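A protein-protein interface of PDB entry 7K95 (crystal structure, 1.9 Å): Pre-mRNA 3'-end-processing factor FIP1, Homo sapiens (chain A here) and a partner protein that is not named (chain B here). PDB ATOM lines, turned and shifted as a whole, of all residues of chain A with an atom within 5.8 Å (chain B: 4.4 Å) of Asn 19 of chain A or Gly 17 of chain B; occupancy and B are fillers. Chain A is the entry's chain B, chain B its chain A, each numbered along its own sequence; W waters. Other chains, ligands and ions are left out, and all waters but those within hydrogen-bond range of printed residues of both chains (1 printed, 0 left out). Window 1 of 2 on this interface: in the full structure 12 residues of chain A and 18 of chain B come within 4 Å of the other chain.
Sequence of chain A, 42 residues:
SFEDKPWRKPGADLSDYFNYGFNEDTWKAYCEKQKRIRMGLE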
ATOM      1  N   LEU A  14      -2.938   5.679  24.135  1.00  0.00           N
ATOM      2  CA  LEU A  14      -4.085   6.620  24.243  1.00  0.00           C
ATOM      3  C   LEU A  14      -3.771   7.711  25.273  1.00  0.00           C
ATOM      4  O   LEU A  14      -4.190   8.875  25.103  1.00  0.00           O
ATOM      5  CB  LEU A  14      -5.322   5.823  24.657  1.00  0.00           C
ATOM      6  CG  LEU A  14      -6.335   5.577  23.546  1.00  0.00           C
ATOM      7  CD1 LEU A  14      -7.360   4.522  23.956  1.00  0.00           C
ATOM      8  CD2 LEU A  14      -7.017   6.883  23.191  1.00  0.00           C
ATOM      9  N   SER A  15      -3.050   7.314  26.303  1.00  0.00           N
ATOM     10  CA  SER A  15      -2.636   8.118  27.478  1.00  0.00           C
ATOM     11  C   SER A  15      -1.615   9.209  27.062  1.00  0.00           C
ATOM     12  O   SER A  15      -1.404  10.123  27.818  1.00  0.00           O
ATOM     13  CB  SER A  15      -2.073   7.178  28.516  1.00  0.00           C
ATOM     14  OG  SER A  15      -0.699   6.902  28.274  1.00  0.00           O
ATOM     15  N   TYR A  17      -2.271  11.164  24.727  1.00  0.00           N
ATOM     16  CA  TYR A  17      -3.246  12.109  24.130  1.00  0.00           C
ATOM     17  C   TYR A  17      -4.265  12.524  25.191  1.00  0.00           C
ATOM     18  O   TYR A  17      -4.591  13.685  25.271  1.00  0.00           O
ATOM     19  CB  TYR A  17      -3.889  11.445  22.912  1.00  0.00           C
ATOM     20  CG  TYR A  17      -2.964  11.199  21.743  1.00  0.00           C
ATOM     21  CD1 TYR A  17      -2.190  10.049  21.651  1.00  0.00           C
ATOM     22  CD2 TYR A  17      -2.931  12.093  20.674  1.00  0.00           C
ATOM     23  CE1 TYR A  17      -1.328   9.839  20.569  1.00  0.00           C
ATOM     24  CE2 TYR A  17      -2.111  11.880  19.572  1.00  0.00           C
ATOM     25  CZ  TYR A  17      -1.317  10.750  19.523  1.00  0.00           C
ATOM     26  OH  TYR A  17      -0.570  10.582  18.407  1.00  0.00           O
ATOM     27  N   PHE A  18      -4.753  11.558  25.952  1.00  0.00           N
ATOM     28  CA  PHE A  18      -5.817  11.752  26.951  1.00  0.00           C
ATOM     29  C   PHE A  18      -5.262  11.579  28.349  1.00  0.00           C
ATOM     30  O   PHE A  18      -4.593  10.560  28.627  1.00  0.00           O
ATOM     31  CB  PHE A  18      -6.909  10.737  26.692  1.00  0.00           C
ATOM     32  CG  PHE A  18      -7.629  10.982  25.408  1.00  0.00           C
ATOM     33  CD1 PHE A  18      -8.617  11.956  25.337  1.00  0.00           C
ATOM     34  CD2 PHE A  18      -7.278  10.273  24.263  1.00  0.00           C
ATOM     35  CE1 PHE A  18      -9.282  12.187  24.151  1.00  0.00           C
ATOM     36  CE2 PHE A  18      -7.942  10.520  23.079  1.00  0.00           C
ATOM     37  CZ  PHE A  18      -8.959  11.460  23.035  1.00  0.00           C
ATOM     38  N   ASN A  19      -5.637  12.512  29.222  1.00  0.00           N
ATOM     39  CA  ASN A  19      -5.258  12.513  30.656  1.00  0.00           C
ATOM     40  C   ASN A  19      -6.396  11.881  31.451  1.00  0.00           C
ATOM     41  O   ASN A  19      -7.514  11.629  30.871  1.00  0.00           O
ATOM     42  CB  ASN A  19      -4.799  13.890  31.127  1.00  0.00           C
ATOM     43  CG  ASN A  19      -3.891  13.915  32.341  1.00  0.00           C
ATOM     44  OD1 ASN A  19      -3.670  12.866  32.965  1.00  0.00           O
ATOM     45  ND2 ASN A  19      -3.474  15.118  32.718  1.00  0.00           N
ATOM     46  N   TYR A  20      -6.137  11.599  32.713  1.00  0.00           N
ATOM     47  CA  TYR A  20      -7.169  11.188  33.705  1.00  0.00           C
ATOM     48  C   TYR A  20      -7.813   9.841  33.365  1.00  0.00           C
ATOM     49  O   TYR A  20      -8.782   9.511  34.066  1.00  0.00           O
ATOM     50  CB  TYR A  20      -8.304  12.218  33.818  1.00  0.00           C
ATOM     51  CG  TYR A  20      -7.723  13.587  34.041  1.00  0.00           C
ATOM     52  CD1 TYR A  20      -7.083  13.860  35.210  1.00  0.00           C
ATOM     53  CD2 TYR A  20      -7.759  14.567  33.078  1.00  0.00           C
ATOM     54  CE1 TYR A  20      -6.498  15.069  35.419  1.00  0.00           C
ATOM     55  CE2 TYR A  20      -7.165  15.798  33.272  1.00  0.00           C
ATOM     56  CZ  TYR A  20      -6.500  16.032  34.437  1.00  0.00           C
ATOM     57  OH  TYR A  20      -5.857  17.198  34.674  1.00  0.00           O
ATOM     58  N   GLY A  21      -7.316   9.070  32.399  1.00  0.00           N
ATOM     59  CA  GLY A  21      -8.013   7.838  32.012  1.00  0.00           C
ATOM     60  C   GLY A  21      -9.145   8.087  31.033  1.00  0.00           C
ATOM     61  O   GLY A  21      -9.892   7.157  30.741  1.00  0.00           O
ATOM     62  N   PHE A  22      -9.290   9.282  30.482  1.00  0.00           N
ATOM     63  CA  PHE A  22     -10.290   9.528  29.414  1.00  0.00           C
ATOM     64  C   PHE A  22      -9.962   8.712  28.149  1.00  0.00           C
ATOM     65  O   PHE A  22      -8.776   8.428  27.857  1.00  0.00           O
ATOM     66  CB  PHE A  22     -10.271  10.981  29.018  1.00  0.00           C
ATOM     67  CG  PHE A  22     -11.047  11.882  29.937  1.00  0.00           C
ATOM     68  CD1 PHE A  22     -12.412  11.711  30.091  1.00  0.00           C
ATOM     69  CD2 PHE A  22     -10.430  12.950  30.575  1.00  0.00           C
ATOM     70  CE1 PHE A  22     -13.143  12.558  30.915  1.00  0.00           C
ATOM     71  CE2 PHE A  22     -11.165  13.813  31.356  1.00  0.00           C
ATOM     72  CZ  PHE A  22     -12.504  13.598  31.545  1.00  0.00           C
ATOM     73  N   TRP A  27     -14.141  11.509  26.803  1.00  0.00           N
ATOM     74  CA  TRP A  27     -13.735  12.913  26.602  1.00  0.00           C
ATOM     75  C   TRP A  27     -14.903  13.691  25.967  1.00  0.00           C
ATOM     76  O   TRP A  27     -15.286  14.780  26.461  1.00  0.00           O
ATOM     77  CB  TRP A  27     -12.438  12.999  25.768  1.00  0.00           C
ATOM     78  CG  TRP A  27     -12.057  14.422  25.506  1.00  0.00           C
ATOM     79  CD1 TRP A  27     -12.130  15.107  24.323  1.00  0.00           C
ATOM     80  CD2 TRP A  27     -11.683  15.398  26.499  1.00  0.00           C
ATOM     81  NE1 TRP A  27     -11.778  16.423  24.505  1.00  0.00           N
ATOM     82  CE2 TRP A  27     -11.464  16.617  25.826  1.00  0.00           C
ATOM     83  CE3 TRP A  27     -11.399  15.324  27.863  1.00  0.00           C
ATOM     84  CZ2 TRP A  27     -11.052  17.764  26.498  1.00  0.00           C
ATOM     85  CZ3 TRP A  27     -11.023  16.472  28.531  1.00  0.00           C
ATOM     86  CH2 TRP A  27     -10.868  17.678  27.857  1.00  0.00           C
ATOM     87  N   TRP B  13      -2.870  21.806  27.564  1.00  0.00           N
ATOM     88  CA  TRP B  13      -3.909  21.017  26.836  1.00  0.00           C
ATOM     89  C   TRP B  13      -4.057  19.657  27.509  1.00  0.00           C
ATOM     90  O   TRP B  13      -5.162  19.248  27.885  1.00  0.00           O
ATOM     91  CB  TRP B  13      -3.611  20.907  25.335  1.00  0.00           C
ATOM     92  CG  TRP B  13      -3.799  22.201  24.594  1.00  0.00           C
ATOM     93  CD1 TRP B  13      -4.950  22.671  24.042  1.00  0.00           C
ATOM     94  CD2 TRP B  13      -2.784  23.201  24.330  1.00  0.00           C
ATOM     95  NE1 TRP B  13      -4.729  23.910  23.494  1.00  0.00           N
ATOM     96  CE2 TRP B  13      -3.427  24.279  23.672  1.00  0.00           C
ATOM     97  CE3 TRP B  13      -1.419  23.337  24.648  1.00  0.00           C
ATOM     98  CZ2 TRP B  13      -2.717  25.426  23.257  1.00  0.00           C
ATOM     99  CZ3 TRP B  13      -0.717  24.486  24.303  1.00  0.00           C
ATOM    100  CH2 TRP B  13      -1.360  25.509  23.581  1.00  0.00           C
ATOM    101  N   TYR B  14      -2.956  18.983  27.789  1.00  0.00           N
ATOM    102  CA  TYR B  14      -2.994  17.656  28.461  1.00  0.00           C
ATOM    103  C   TYR B  14      -3.634  17.805  29.850  1.00  0.00           C
ATOM    104  O   TYR B  14      -4.371  16.887  30.264  1.00  0.00           O
ATOM    105  CB  TYR B  14      -1.595  17.022  28.517  1.00  0.00           C
ATOM    106  CG  TYR B  14      -1.639  15.554  28.886  1.00  0.00           C
ATOM    107  CD1 TYR B  14      -2.073  14.586  27.991  1.00  0.00           C
ATOM    108  CD2 TYR B  14      -1.304  15.146  30.166  1.00  0.00           C
ATOM    109  CE1 TYR B  14      -2.139  13.239  28.341  1.00  0.00           C
ATOM    110  CE2 TYR B  14      -1.349  13.810  30.529  1.00  0.00           C
ATOM    111  CZ  TYR B  14      -1.780  12.855  29.626  1.00  0.00           C
ATOM    112  OH  TYR B  14      -1.716  11.542  30.008  1.00  0.00           O
ATOM    113  N   ASP B  15      -3.310  18.896  30.580  1.00  0.00           N
ATOM    114  CA  ASP B  15      -3.844  19.175  31.926  1.00  0.00           C
ATOM    115  C   ASP B  15      -5.377  19.400  31.872  1.00  0.00           C
ATOM    116  O   ASP B  15      -6.069  19.002  32.807  1.00  0.00           O
ATOM    117  CB  ASP B  15      -3.193  20.365  32.561  1.00  0.00           C
ATOM    118  CG  ASP B  15      -1.778  20.026  33.069  1.00  0.00           C
ATOM    119  OD1 ASP B  15      -1.443  18.842  33.108  1.00  0.00           O
ATOM    120  OD2 ASP B  15      -1.182  20.912  33.551  1.00  0.00           O
ATOM    121  N   ARG B  16      -5.874  19.962  30.792  1.00  0.00           N
ATOM    122  CA  ARG B  16      -7.357  20.117  30.577  1.00  0.00           C
ATOM    123  C   ARG B  16      -7.926  18.729  30.247  1.00  0.00           C
ATOM    124  O   ARG B  16      -9.082  18.400  30.763  1.00  0.00           O
ATOM    125  CB  ARG B  16      -7.585  21.143  29.451  1.00  0.00           C
ATOM    126  CG  ARG B  16      -9.029  21.197  28.935  1.00  0.00           C
ATOM    127  CD  ARG B  16      -9.158  22.331  27.912  1.00  0.00           C
ATOM    128  NE  ARG B  16     -10.468  22.529  27.305  1.00  0.00           N
ATOM    129  CZ  ARG B  16     -10.860  21.942  26.221  1.00  0.00           C
ATOM    130  NH1 ARG B  16     -10.062  21.061  25.643  1.00  0.00           N
ATOM    131  NH2 ARG B  16     -12.023  22.230  25.662  1.00  0.00           N
ATOM    132  N   GLY B  17      -7.136  17.866  29.566  1.00  0.00           N
ATOM    133  CA  GLY B  17      -7.470  16.430  29.454  1.00  0.00           C
ATOM    134  C   GLY B  17      -7.161  15.785  28.115  1.00  0.00           C
ATOM    135  O   GLY B  17      -7.103  14.523  28.037  1.00  0.00           O
ATOM    136  N   PHE B  18      -6.960  16.599  27.100  1.00  0.00           N
ATOM    137  CA  PHE B  18      -6.715  16.124  25.722  1.00  0.00           C
ATOM    138  C   PHE B  18      -5.663  17.003  25.036  1.00  0.00           C
ATOM    139  O   PHE B  18      -5.901  18.196  24.888  1.00  0.00           O
ATOM    140  CB  PHE B  18      -8.031  16.105  24.945  1.00  0.00           C
ATOM    141  CG  PHE B  18      -7.803  15.852  23.486  1.00  0.00           C
ATOM    142  CD1 PHE B  18      -7.336  14.631  23.062  1.00  0.00           C
ATOM    143  CD2 PHE B  18      -7.923  16.879  22.559  1.00  0.00           C
ATOM    144  CE1 PHE B  18      -7.075  14.401  21.723  1.00  0.00           C
ATOM    145  CE2 PHE B  18      -7.671  16.649  21.201  1.00  0.00           C
ATOM    146  CZ  PHE B  18      -7.234  15.405  20.791  1.00  0.00           C
ATOM    147  N   THR B  30       1.954  15.191  31.917  1.00  0.00           N
ATOM    148  CA  THR B  30       1.977  14.692  33.323  1.00  0.00           C
ATOM    149  C   THR B  30       0.698  13.911  33.578  1.00  0.00           C
ATOM    150  O   THR B  30      -0.367  14.559  33.593  1.00  0.00           O
ATOM    151  CB  THR B  30       2.205  15.823  34.330  1.00  0.00           C
ATOM    152  OG1 THR B  30       3.519  16.320  34.065  1.00  0.00           O
ATOM    153  CG2 THR B  30       2.118  15.301  35.751  1.00  0.00           C
ATOM    154  N   ARG B  31       0.785  12.580  33.762  1.00  0.00           N
ATOM    155  CA  ARG B  31      -0.467  11.809  34.035  1.00  0.00           C
ATOM    156  C   ARG B  31      -0.972  12.190  35.417  1.00  0.00           C
ATOM    157  O   ARG B  31      -0.185  12.218  36.397  1.00  0.00           O
ATOM    158  CB  ARG B  31      -0.217  10.300  33.963  1.00  0.00           C
ATOM    159  CG  ARG B  31      -0.257   9.759  32.539  1.00  0.00           C
ATOM    160  CD  ARG B  31       0.826  10.246  31.613  1.00  0.00           C
ATOM    161  NE  ARG B  31       0.961   9.372  30.466  1.00  0.00           N
ATOM    162  CZ  ARG B  31       1.481   9.707  29.301  1.00  0.00           C
ATOM    163  NH1 ARG B  31       1.939  10.932  29.092  1.00  0.00           N
ATOM    164  NH2 ARG B  31       1.508   8.831  28.327  1.00  0.00           N
ATOM    165  N   ARG B  32      -2.251  12.496  35.503  1.00  0.00           N
ATOM    166  CA  ARG B  32      -2.900  12.870  36.759  1.00  0.00           C
ATOM    167  C   ARG B  32      -4.215  12.102  36.924  1.00  0.00           C
ATOM    168  O   ARG B  32      -4.684  11.480  35.961  1.00  0.00           O
ATOM    169  CB  ARG B  32      -3.220  14.358  36.761  1.00  0.00           C
ATOM    170  CG  ARG B  32      -1.992  15.257  36.585  1.00  0.00           C
ATOM    171  CD  ARG B  32      -2.391  16.730  36.495  1.00  0.00           C
ATOM    172  NE  ARG B  32      -1.250  17.608  36.129  1.00  0.00           N
ATOM    173  CZ  ARG B  32      -0.433  18.177  37.007  1.00  0.00           C
ATOM    174  NH1 ARG B  32      -0.585  17.979  38.299  1.00  0.00           N
ATOM    175  NH2 ARG B  32       0.516  18.978  36.592  1.00  0.00           N
HETATM  176  O   HOH W   1       0.801   6.718  31.177  1.00  0.00           O
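O of Trp 13 of chain B is in hydrogen-bond range of N of Phe 18 of chain B (3.3 Å). The guanidinium group (NE) of Arg 31 of chain B sits close to the side-chain hydroxyl (OH) of Tyr 14 of chain B (3.5 Å). NE of Arg 32 of chain B is in salt-bridge range of OD1 of Asp 15 of chain B (3.3 Å).
Printed residues of chain B within 4 Å of Ser 15 of chain A: Tyr 14 (2.6 Å) and Arg 31 (2.9 Å). Asn 19 of chain A touches just these residues of chain B: Tyr 14 (3.1 Å), Gly 17 (2.8 Å), Thr 30 (3.3 Å), Arg 31 (3.5 Å) and Arg 32 (2.9 Å). Printed residues of chain A within 4 Å of Asp 15 of chain B: Tyr 20. Of the printed residues of chain A, Arg 16 of chain B touches Trp 27. Printed residues of chain A within 4 Å of Gly 17 of chain B: Tyr 17, Phe 18, Asn 19, Tyr 20 and Trp 27. Of the printed residues of chain A, Phe 18 of chain B touches Tyr 17 (3.3 Å), Phe 18 (3.3 Å) and Trp 27 (3.6 Å). Printed residues of chain A within 4 Å of Arg 31 of chain B: Ser 15 (2.9 Å) and Asn 19 (3.5 Å). The nearest printed residue of chain B that does not touch Ser 15 of chain A is Gly 17 of chain B (7.2 Å).
OH of Tyr 14 of chain B is in hydrogen-bond range of O of Ser 15 of chain A (2.6 Å). The side-chain hydroxyl of Tyr 14 of chain B lies within hydrogen-bond range of the backbone carbonyl oxygen of Phe 18 of chain A, 3.3 Å away. The backbone carbonyl oxygen of Tyr 14 of chain B sits close to the side-chain amide nitrogen of Asn 19 of chain A. The backbone carbonyl oxygen (O) of Asp 15 of chain B lies within hydrogen-bond range of the side-chain hydroxyl (OH) of Tyr 20 of chain A. The backbone carbonyl oxygen (O) of Gly 17 of chain B lies within hydrogen-bond range of the backbone NH (N) of Asn 19 of chain A (2.8 Å). The backbone carbonyl oxygen of Thr 30 of chain B sits at hydrogen-bond distance from the side-chain amide nitrogen of Asn 19 of chain A (3.3 Å). The side-chain hydroxyl (OG) of Ser 15 of chain A is in hydrogen-bond range of the guanidinium group (NH2) of Arg 31 of chain B (2.9 Å). The side-chain amide oxygen (OD1) of Asn 19 of chain A lies within hydrogen-bond range of the backbone NH (N) of Arg 32 of chain B, at 2.9 Å.
Water W1 bridges NE of Arg 31 of chain B (2.8 Å) and OG of Ser 15 of chain A (3.3 Å).
Among the printed residues, pairs that only touch across the chains: Tyr 17 of chain A with Tyr 14 of chain B (3.8 Å), Tyr 17 of chain A with Gly 17 of chain B (3.8 Å), Tyr 17 of chain A with Phe 18 of chain B (3.3 Å), Phe 18 of chain A with Gly 17 of chain B (3.2 Å), Phe 18 of chain A with Phe 18 of chain B (3.3 Å), Asn 19 of chain A with Arg 31 of chain B (3.5 Å), Tyr 20 of chain A with Gly 17 of chain B (3.9 Å), Tyr 20 of chain A with Arg 32 of chain B (3.4 Å), Trp 27 of chain A with Arg 16 of chain B (3.5 Å), Trp 27 of chain A with Gly 17 of chain B (3.7 Å) and Trp 27 of chain A with Phe 18 of chain B (3.6 Å).
Of the 9 printed residues of chain B, 8 touch a printed residue of chain A. Hydrophobic or aromatic side chains of chain B that line the printed part of chain A: Tyr 14 and Phe 18. Among the printed residues, 19 pairs touch across the chains. Among the printed residues, no Asp or Glu carboxylate lies within 4 Å of a Lys or Arg side-chain nitrogen of the other chain.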
